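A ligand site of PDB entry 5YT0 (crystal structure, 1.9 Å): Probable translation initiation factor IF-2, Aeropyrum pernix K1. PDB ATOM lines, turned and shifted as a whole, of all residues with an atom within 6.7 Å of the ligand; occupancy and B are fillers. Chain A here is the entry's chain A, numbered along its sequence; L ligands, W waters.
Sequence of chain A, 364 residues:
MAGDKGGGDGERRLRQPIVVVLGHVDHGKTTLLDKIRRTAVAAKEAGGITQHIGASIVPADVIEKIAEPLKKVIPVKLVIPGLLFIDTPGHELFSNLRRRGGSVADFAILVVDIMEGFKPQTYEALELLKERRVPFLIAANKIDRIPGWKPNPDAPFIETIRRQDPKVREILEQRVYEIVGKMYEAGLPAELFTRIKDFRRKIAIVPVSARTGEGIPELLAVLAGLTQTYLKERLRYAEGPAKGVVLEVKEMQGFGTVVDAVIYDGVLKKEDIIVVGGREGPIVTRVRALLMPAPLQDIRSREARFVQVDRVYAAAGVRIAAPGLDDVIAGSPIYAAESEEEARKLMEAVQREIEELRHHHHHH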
ATOM      1  N   GLY A  23      -4.700  -0.062  19.387  1.00  0.00           N
ATOM      2  CA  GLY A  23      -5.182  -0.388  18.067  1.00  0.00           C
ATOM      3  C   GLY A  23      -4.500  -1.633  17.488  1.00  0.00           C
ATOM      4  O   GLY A  23      -3.522  -2.177  18.066  1.00  0.00           O
ATOM      5  N   HIS A  24      -5.011  -2.071  16.319  1.00  0.00           N
ATOM      6  CA  HIS A  24      -4.484  -3.344  15.721  1.00  0.00           C
ATOM      7  C   HIS A  24      -3.097  -3.251  15.196  1.00  0.00           C
ATOM      8  O   HIS A  24      -2.572  -2.226  14.708  1.00  0.00           O
ATOM      9  CB  HIS A  24      -5.507  -3.829  14.670  1.00  0.00           C
ATOM     10  CG  HIS A  24      -5.310  -5.222  14.218  1.00  0.00           C
ATOM     11  ND1 HIS A  24      -5.981  -6.270  14.799  1.00  0.00           N
ATOM     12  CD2 HIS A  24      -4.671  -5.714  13.170  1.00  0.00           C
ATOM     13  CE1 HIS A  24      -5.682  -7.400  14.175  1.00  0.00           C
ATOM     14  NE2 HIS A  24      -4.889  -7.093  13.183  1.00  0.00           N
ATOM     15  N   VAL A  25      -2.411  -4.412  15.300  1.00  0.00           N
ATOM     16  CA  VAL A  25      -1.152  -4.485  14.703  1.00  0.00           C
ATOM     17  C   VAL A  25      -1.033  -4.004  13.281  1.00  0.00           C
ATOM     18  O   VAL A  25      -1.833  -4.283  12.413  1.00  0.00           O
ATOM     19  CB  VAL A  25      -0.522  -6.000  14.965  1.00  0.00           C
ATOM     20  CG1 VAL A  25      -1.383  -6.997  14.275  1.00  0.00           C
ATOM     21  CG2 VAL A  25       0.930  -6.044  14.386  1.00  0.00           C
ATOM     22  N   ASP A  26      -0.035  -3.210  13.024  1.00  0.00           N
ATOM     23  CA  ASP A  26       0.319  -2.612  11.759  1.00  0.00           C
ATOM     24  C   ASP A  26      -0.587  -1.418  11.402  1.00  0.00           C
ATOM     25  O   ASP A  26      -0.364  -0.832  10.315  1.00  0.00           O
ATOM     26  CB  ASP A  26       0.342  -3.577  10.559  1.00  0.00           C
ATOM     27  CG  ASP A  26       1.712  -3.859  10.108  1.00  0.00           C
ATOM     28  OD1 ASP A  26       2.500  -4.424  10.910  1.00  0.00           O
ATOM     29  OD2 ASP A  26       2.032  -3.416   8.972  1.00  0.00           O
ATOM     30  N   HIS A  27      -1.435  -0.986  12.336  1.00  0.00           N
ATOM     31  CA  HIS A  27      -2.314   0.193  11.967  1.00  0.00           C
ATOM     32  C   HIS A  27      -1.634   1.559  12.131  1.00  0.00           C
ATOM     33  O   HIS A  27      -2.086   2.547  11.633  1.00  0.00           O
ATOM     34  CB  HIS A  27      -3.627   0.021  12.769  1.00  0.00           C
ATOM     35  CG  HIS A  27      -4.530  -0.962  12.132  1.00  0.00           C
ATOM     36  ND1 HIS A  27      -5.888  -0.882  12.239  1.00  0.00           N
ATOM     37  CD2 HIS A  27      -4.269  -2.011  11.289  1.00  0.00           C
ATOM     38  CE1 HIS A  27      -6.446  -1.916  11.613  1.00  0.00           C
ATOM     39  NE2 HIS A  27      -5.481  -2.616  11.043  1.00  0.00           N
ATOM     40  N   GLY A  28      -0.453   1.543  12.787  1.00  0.00           N
ATOM     41  CA  GLY A  28       0.404   2.718  12.843  1.00  0.00           C
ATOM     42  C   GLY A  28       0.628   3.289  14.221  1.00  0.00           C
ATOM     43  O   GLY A  28       1.042   4.468  14.299  1.00  0.00           O
ATOM     44  N   LYS A  29       0.510   2.473  15.327  1.00  0.00           N
ATOM     45  CA  LYS A  29       0.650   3.023  16.613  1.00  0.00           C
ATOM     46  C   LYS A  29       2.041   3.618  16.854  1.00  0.00           C
ATOM     47  O   LYS A  29       2.220   4.752  17.384  1.00  0.00           O
ATOM     48  CB  LYS A  29       0.257   1.961  17.701  1.00  0.00           C
ATOM     49  CG  LYS A  29      -1.162   1.461  17.630  1.00  0.00           C
ATOM     50  CD  LYS A  29      -1.435   0.390  18.673  1.00  0.00           C
ATOM     51  CE  LYS A  29      -0.486  -0.831  18.620  1.00  0.00           C
ATOM     52  NZ  LYS A  29      -0.649  -1.576  17.421  1.00  0.00           N
ATOM     53  N   THR A  30       3.030   2.745  16.638  1.00  0.00           N
ATOM     54  CA  THR A  30       4.433   3.149  16.836  1.00  0.00           C
ATOM     55  C   THR A  30       4.820   4.349  16.053  1.00  0.00           C
ATOM     56  O   THR A  30       5.519   5.259  16.547  1.00  0.00           O
ATOM     57  CB  THR A  30       5.325   1.931  16.576  1.00  0.00           C
ATOM     58  OG1 THR A  30       4.869   0.911  17.368  1.00  0.00           O
ATOM     59  CG2 THR A  30       6.725   2.261  16.943  1.00  0.00           C
ATOM     60  N   THR A  31       4.377   4.341  14.799  1.00  0.00           N
ATOM     61  CA  THR A  31       4.624   5.435  13.857  1.00  0.00           C
ATOM     62  C   THR A  31       4.016   6.753  14.280  1.00  0.00           C
ATOM     63  O   THR A  31       4.658   7.776  14.250  1.00  0.00           O
ATOM     64  CB  THR A  31       4.276   5.092  12.362  1.00  0.00           C
ATOM     65  OG1 THR A  31       5.001   3.897  12.061  1.00  0.00           O
ATOM     66  CG2 THR A  31       4.765   6.168  11.483  1.00  0.00           C
ATOM     67  N   LEU A  32       2.786   6.696  14.702  1.00  0.00           N
ATOM     68  CA  LEU A  32       2.096   7.854  15.200  1.00  0.00           C
ATOM     69  C   LEU A  32       2.812   8.427  16.421  1.00  0.00           C
ATOM     70  O   LEU A  32       3.031   9.660  16.508  1.00  0.00           O
ATOM     71  CB  LEU A  32       0.639   7.529  15.566  1.00  0.00           C
ATOM     72  CG  LEU A  32      -0.131   8.832  16.037  1.00  0.00           C
ATOM     73  CD1 LEU A  32      -0.232   9.820  14.898  1.00  0.00           C
ATOM     74  CD2 LEU A  32      -1.569   8.295  16.226  1.00  0.00           C
ATOM     75  N   PRO A  89       2.924   1.208  23.015  1.00  0.00           N
ATOM     76  CA  PRO A  89       1.478   1.110  22.692  1.00  0.00           C
ATOM     77  C   PRO A  89       0.949  -0.267  22.932  1.00  0.00           C
ATOM     78  O   PRO A  89       1.749  -1.279  23.133  1.00  0.00           O
ATOM     79  CB  PRO A  89       1.454   1.424  21.239  1.00  0.00           C
ATOM     80  CG  PRO A  89       2.710   1.008  20.673  1.00  0.00           C
ATOM     81  CD  PRO A  89       3.765   1.118  21.807  1.00  0.00           C
ATOM     82  N   VAL A 111      -6.062   3.868  17.323  1.00  0.00           N
ATOM     83  CA  VAL A 111      -5.516   4.043  16.010  1.00  0.00           C
ATOM     84  C   VAL A 111      -6.242   3.015  15.187  1.00  0.00           C
ATOM     85  O   VAL A 111      -6.279   1.821  15.598  1.00  0.00           O
ATOM     86  CB  VAL A 111      -4.027   3.828  15.992  1.00  0.00           C
ATOM     87  CG1 VAL A 111      -3.451   3.944  14.500  1.00  0.00           C
ATOM     88  CG2 VAL A 111      -3.294   4.884  16.821  1.00  0.00           C
ATOM     89  N   ASP A 113      -6.355   1.982  10.974  1.00  0.00           N
ATOM     90  CA  ASP A 113      -5.850   2.197   9.594  1.00  0.00           C
ATOM     91  C   ASP A 113      -7.123   2.411   8.756  1.00  0.00           C
ATOM     92  O   ASP A 113      -7.988   1.577   8.616  1.00  0.00           O
ATOM     93  CB  ASP A 113      -5.110   0.956   9.135  1.00  0.00           C
ATOM     94  CG  ASP A 113      -4.538   1.049   7.646  1.00  0.00           C
ATOM     95  OD1 ASP A 113      -4.961   1.818   6.725  1.00  0.00           O
ATOM     96  OD2 ASP A 113      -3.582   0.268   7.439  1.00  0.00           O
ATOM     97  N   ASN A 141      -5.839   6.624  10.722  1.00  0.00           N
ATOM     98  CA  ASN A 141      -4.467   6.821  10.239  1.00  0.00           C
ATOM     99  C   ASN A 141      -4.267   6.317   8.797  1.00  0.00           C
ATOM    100  O   ASN A 141      -5.137   5.596   8.281  1.00  0.00           O
ATOM    101  CB  ASN A 141      -3.526   6.017  11.154  1.00  0.00           C
ATOM    102  CG  ASN A 141      -2.078   6.355  10.891  1.00  0.00           C
ATOM    103  OD1 ASN A 141      -1.708   7.518  10.521  1.00  0.00           O
ATOM    104  ND2 ASN A 141      -1.214   5.307  11.031  1.00  0.00           N
ATOM    105  N   LYS A 142      -3.160   6.683   8.192  1.00  0.00           N
ATOM    106  CA  LYS A 142      -2.774   6.287   6.786  1.00  0.00           C
ATOM    107  C   LYS A 142      -3.694   6.969   5.717  1.00  0.00           C
ATOM    108  O   LYS A 142      -3.849   6.427   4.560  1.00  0.00           O
ATOM    109  CB  LYS A 142      -2.689   4.812   6.577  1.00  0.00           C
ATOM    110  CG  LYS A 142      -1.904   4.124   7.751  1.00  0.00           C
ATOM    111  CD  LYS A 142      -1.289   2.845   7.270  1.00  0.00           C
ATOM    112  CE  LYS A 142      -0.818   1.961   8.436  1.00  0.00           C
ATOM    113  NZ  LYS A 142      -0.211   0.796   7.826  1.00  0.00           N
ATOM    114  N   ILE A 143      -4.168   8.190   6.054  1.00  0.00           N
ATOM    115  CA  ILE A 143      -5.020   8.852   5.045  1.00  0.00           C
ATOM    116  C   ILE A 143      -4.167   9.093   3.741  1.00  0.00           C
ATOM    117  O   ILE A 143      -4.741   9.212   2.673  1.00  0.00           O
ATOM    118  CB  ILE A 143      -5.564  10.240   5.470  1.00  0.00           C
ATOM    119  CG1 ILE A 143      -4.484  11.209   5.882  1.00  0.00           C
ATOM    120  CG2 ILE A 143      -6.517  10.034   6.623  1.00  0.00           C
ATOM    121  CD1 ILE A 143      -4.959  12.539   6.491  1.00  0.00           C
ATOM    122  N   ASP A 144      -2.826   9.217   3.860  1.00  0.00           N
ATOM    123  CA  ASP A 144      -1.900   9.317   2.713  1.00  0.00           C
ATOM    124  C   ASP A 144      -1.974   8.181   1.693  1.00  0.00           C
ATOM    125  O   ASP A 144      -1.468   8.323   0.622  1.00  0.00           O
ATOM    126  CB  ASP A 144      -0.465   9.669   3.163  1.00  0.00           C
ATOM    127  CG  ASP A 144       0.157   8.517   3.788  1.00  0.00           C
ATOM    128  OD1 ASP A 144      -0.316   8.168   4.912  1.00  0.00           O
ATOM    129  OD2 ASP A 144       0.804   7.728   3.131  1.00  0.00           O
ATOM    130  N   ARG A 145      -2.518   7.052   2.065  1.00  0.00           N
ATOM    131  CA  ARG A 145      -2.715   5.854   1.282  1.00  0.00           C
ATOM    132  C   ARG A 145      -4.083   5.876   0.541  1.00  0.00           C
ATOM    133  O   ARG A 145      -4.342   4.990  -0.188  1.00  0.00           O
ATOM    134  CB  ARG A 145      -2.597   4.552   2.112  1.00  0.00           C
ATOM    135  CG  ARG A 145      -1.178   4.395   2.673  1.00  0.00           C
ATOM    136  CD  ARG A 145      -0.846   2.990   3.219  1.00  0.00           C
ATOM    137  NE  ARG A 145      -0.672   2.087   2.114  1.00  0.00           N
ATOM    138  CZ  ARG A 145      -1.527   1.130   1.788  1.00  0.00           C
ATOM    139  NH1 ARG A 145      -2.631   0.849   2.524  1.00  0.00           N
ATOM    140  NH2 ARG A 145      -1.250   0.459   0.704  1.00  0.00           N
ATOM    141  N   VAL A 208      -5.627  11.194  10.169  1.00  0.00           N
ATOM    142  CA  VAL A 208      -4.236  11.641  10.277  1.00  0.00           C
ATOM    143  C   VAL A 208      -3.399  10.781   9.315  1.00  0.00           C
ATOM    144  O   VAL A 208      -3.842   9.700   8.877  1.00  0.00           O
ATOM    145  CB  VAL A 208      -3.685  11.492  11.722  1.00  0.00           C
ATOM    146  CG1 VAL A 208      -4.441  12.293  12.689  1.00  0.00           C
ATOM    147  CG2 VAL A 208      -3.594  10.084  12.158  1.00  0.00           C
ATOM    148  N   SER A 209      -2.214  11.259   9.143  1.00  0.00           N
ATOM    149  CA  SER A 209      -1.098  10.408   8.546  1.00  0.00           C
ATOM    150  C   SER A 209       0.140  10.439   9.418  1.00  0.00           C
ATOM    151  O   SER A 209       0.737  11.461   9.685  1.00  0.00           O
ATOM    152  CB  SER A 209      -0.733  10.908   7.165  1.00  0.00           C
ATOM    153  OG  SER A 209       0.405  10.077   6.656  1.00  0.00           O
ATOM    154  N   ALA A 210       0.387   9.316  10.052  1.00  0.00           N
ATOM    155  CA  ALA A 210       1.605   9.196  10.881  1.00  0.00           C
ATOM    156  C   ALA A 210       2.901   9.219  10.022  1.00  0.00           C
ATOM    157  O   ALA A 210       3.955   9.528  10.534  1.00  0.00           O
ATOM    158  CB  ALA A 210       1.535   7.935  11.632  1.00  0.00           C
ATOM    159  N   ARG A 211       2.765   9.016   8.727  1.00  0.00           N
ATOM    160  CA  ARG A 211       3.914   9.252   7.730  1.00  0.00           C
ATOM    161  C   ARG A 211       4.129  10.761   7.519  1.00  0.00           C
ATOM    162  O   ARG A 211       5.190  11.300   7.836  1.00  0.00           O
ATOM    163  CB  ARG A 211       3.635   8.489   6.413  1.00  0.00           C
ATOM    164  CG  ARG A 211       4.815   8.875   5.468  1.00  0.00           C
ATOM    165  CD  ARG A 211       4.665   8.077   4.234  1.00  0.00           C
ATOM    166  NE  ARG A 211       3.651   8.540   3.323  1.00  0.00           N
ATOM    167  CZ  ARG A 211       3.844   9.327   2.256  1.00  0.00           C
ATOM    168  NH1 ARG A 211       4.854  10.163   2.103  1.00  0.00           N
ATOM    169  NH2 ARG A 211       2.821   9.497   1.456  1.00  0.00           N
ATOM    170  N   THR A 212       3.126  11.497   6.989  1.00  0.00           N
ATOM    171  CA  THR A 212       3.320  12.880   6.652  1.00  0.00           C
ATOM    172  C   THR A 212       3.087  13.915   7.658  1.00  0.00           C
ATOM    173  O   THR A 212       3.519  15.010   7.493  1.00  0.00           O
ATOM    174  CB  THR A 212       2.437  13.265   5.506  1.00  0.00           C
ATOM    175  OG1 THR A 212       1.057  13.257   5.937  1.00  0.00           O
ATOM    176  CG2 THR A 212       2.572  12.310   4.429  1.00  0.00           C
HETATM  177  P1  LIG L   1       1.891  -0.648  14.898  1.00  0.00           P
HETATM  178  O1  LIG L   1       2.802  -0.047  15.911  1.00  0.00           O
HETATM  179  O2  LIG L   1       2.044  -2.132  14.860  1.00  0.00           O
HETATM  180  O3  LIG L   1       0.412  -0.256  15.019  1.00  0.00           O
HETATM  181  O4  LIG L   1       2.310  -0.156  13.351  1.00  0.00           O
HETATM  182  P2  LIG L   1       3.569   0.642  12.938  1.00  0.00           P
HETATM  183  O5  LIG L   1       3.729   1.988  13.455  1.00  0.00           O
HETATM  184  O6  LIG L   1       4.669  -0.268  13.071  1.00  0.00           O
HETATM  185  O7  LIG L   1       3.307   0.805  11.359  1.00  0.00           O
HETATM  186  C1  LIG L   1       3.128  -0.326  10.488  1.00  0.00           C
HETATM  187  C2  LIG L   1       3.561   0.009   9.078  1.00  0.00           C
HETATM  188  O8  LIG L   1       2.761   1.068   8.442  1.00  0.00           O
HETATM  189  C3  LIG L   1       4.999   0.401   8.989  1.00  0.00           C
HETATM  190  O9  LIG L   1       5.536   0.042   7.763  1.00  0.00           O
HETATM  191  C4  LIG L   1       4.873   1.916   8.943  1.00  0.00           C
HETATM  192  O10 LIG L   1       5.860   2.583   8.205  1.00  0.00           O
HETATM  193  C5  LIG L   1       3.636   2.114   8.138  1.00  0.00           C
HETATM  194  N1  LIG L   1       2.847   3.346   8.499  1.00  0.00           N
HETATM  195  C6  LIG L   1       2.345   3.693   9.803  1.00  0.00           C
HETATM  196  N2  LIG L   1       1.694   4.874   9.760  1.00  0.00           N
HETATM  197  C7  LIG L   1       1.594   5.178   8.408  1.00  0.00           C
HETATM  198  C8  LIG L   1       0.888   6.131   7.633  1.00  0.00           C
HETATM  199  O11 LIG L   1       0.225   7.027   8.203  1.00  0.00           O
HETATM  200  N3  LIG L   1       1.109   6.144   6.285  1.00  0.00           N
HETATM  201  C9  LIG L   1       1.817   5.200   5.620  1.00  0.00           C
HETATM  202  N4  LIG L   1       1.869   5.304   4.278  1.00  0.00           N
HETATM  203  N5  LIG L   1       2.442   4.172   6.237  1.00  0.00           N
HETATM  204  C10 LIG L   1       2.357   4.179   7.613  1.00  0.00           C
HETATM  205  O   HOH W   1       3.786  -0.413   5.492  1.00  0.00           O
HETATM  206  O   HOH W   2       4.110  -3.156  13.324  1.00  0.00           O
HETATM  207  O   HOH W   3       1.443  -3.486  17.216  1.00  0.00           O
HETATM  208  O   HOH W   4       1.754   1.583   5.161  1.00  0.00           O
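The backbone NH of Thr 31 sits at hydrogen-bond distance from an oxygen (O5) of the ligand, at 2.8 Å.
The side-chain hydroxyl (OG1) of Thr 31 lies within hydrogen-bond range of an oxygen (O5) of the ligand, 2.7 Å away.
The backbone NH of Thr 30 lies within hydrogen-bond range of an oxygen (O1) of the ligand (2.9 Å).
The side-chain hydroxyl (OG1) of Thr 30 sits at hydrogen-bond distance from an oxygen (O1) of the ligand, 2.7 Å away.
O3 of the ligand sits at hydrogen-bond distance from N of Lys 29 (2.7 Å).
The side-chain amino group of Lys 29 is in salt-bridge range of an oxygen (O3) of the ligand (2.9 Å).
The side-chain carboxylate of Asp 144 is in hydrogen-bond range of a nitrogen (N3) of the ligand (2.8 Å).
N of Ala 210 is in hydrogen-bond range of O11 of the ligand (2.9 Å).
The backbone NH (N) of Asp 26 is in hydrogen-bond range of an oxygen (O2) of the ligand, at 3.0 Å.
The backbone NH of Gly 28 is in hydrogen-bond range of an oxygen (O3) of the ligand, at 3.0 Å.
The backbone NH (N) of Lys 142 sits close to an oxygen (O11) of the ligand.
NZ of Lys 142 is in hydrogen-bond range of O8 of the ligand (3.0 Å).
The side-chain amide oxygen of Asn 141 sits close to an oxygen (O11) of the ligand, 3.1 Å away.
An oxygen (O11) of the ligand is in hydrogen-bond range of the backbone NH (N) of Arg 211.
The backbone NH (N) of His 27 is in hydrogen-bond range of an oxygen (O3) of the ligand, at 3.3 Å.
O11 of the ligand is in hydrogen-bond range of OG of Ser 209, at 3.4 Å.
The side-chain amino group (NZ) of Lys 29 sits at hydrogen-bond distance from the backbone carbonyl oxygen (O) of His 24 (3.4 Å).
The side-chain amino group (NZ) of Lys 29 lies within hydrogen-bond range of the backbone carbonyl oxygen (O) of Gly 23, 3.0 Å away.
NE of Arg 211 is in salt-bridge range of OD2 of Asp 144 (3.0 Å).
OD1 of Asn 141 is in hydrogen-bond range of N of Ala 210 (2.8 Å).
The backbone carbonyl oxygen (O) of Asp 26 sits at hydrogen-bond distance from the side-chain amino group (NZ) of Lys 142 (3.0 Å).
The backbone carbonyl oxygen (O) of His 27 is in hydrogen-bond range of the side-chain amide nitrogen (ND2) of Asn 141.
The side-chain amide oxygen (OD1) of Asn 141 lies close to the backbone carbonyl oxygen (O) of Val 208 (3.5 Å).
OG of Ser 209 sits close to N of Arg 211 (3.3 Å).
O of His 24 touches O3 of the ligand, at 3.6 Å.
C of Val 25 touches O2 of the ligand (3.9 Å).
CG of Arg 145 touches N4 of the ligand, 3.6 Å away.
Within 4 Å of the ligand: His 24, Val 25, Asp 26, His 27, Gly 28, Lys 29, Thr 30, Thr 31, Asn 141, Lys 142, Asp 144, Arg 145, Ser 209, Ala 210 and Arg 211.
The nearest printed residue that does not touch the ligand is Pro 89 (4.9 Å).
Water W2 bridges an oxygen (O2) of the ligand (2.8 Å) and the side-chain carboxylate (OD1) of Asp 26 (3.2 Å).
Water W3 bridges O2 of the ligand (2.8 Å) and NZ of Lys 29 (2.8 Å).
Water W4 bridges a nitrogen (N5) of the ligand (2.9 Å) and the side-chain amino group of Lys 142 (3.4 Å).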
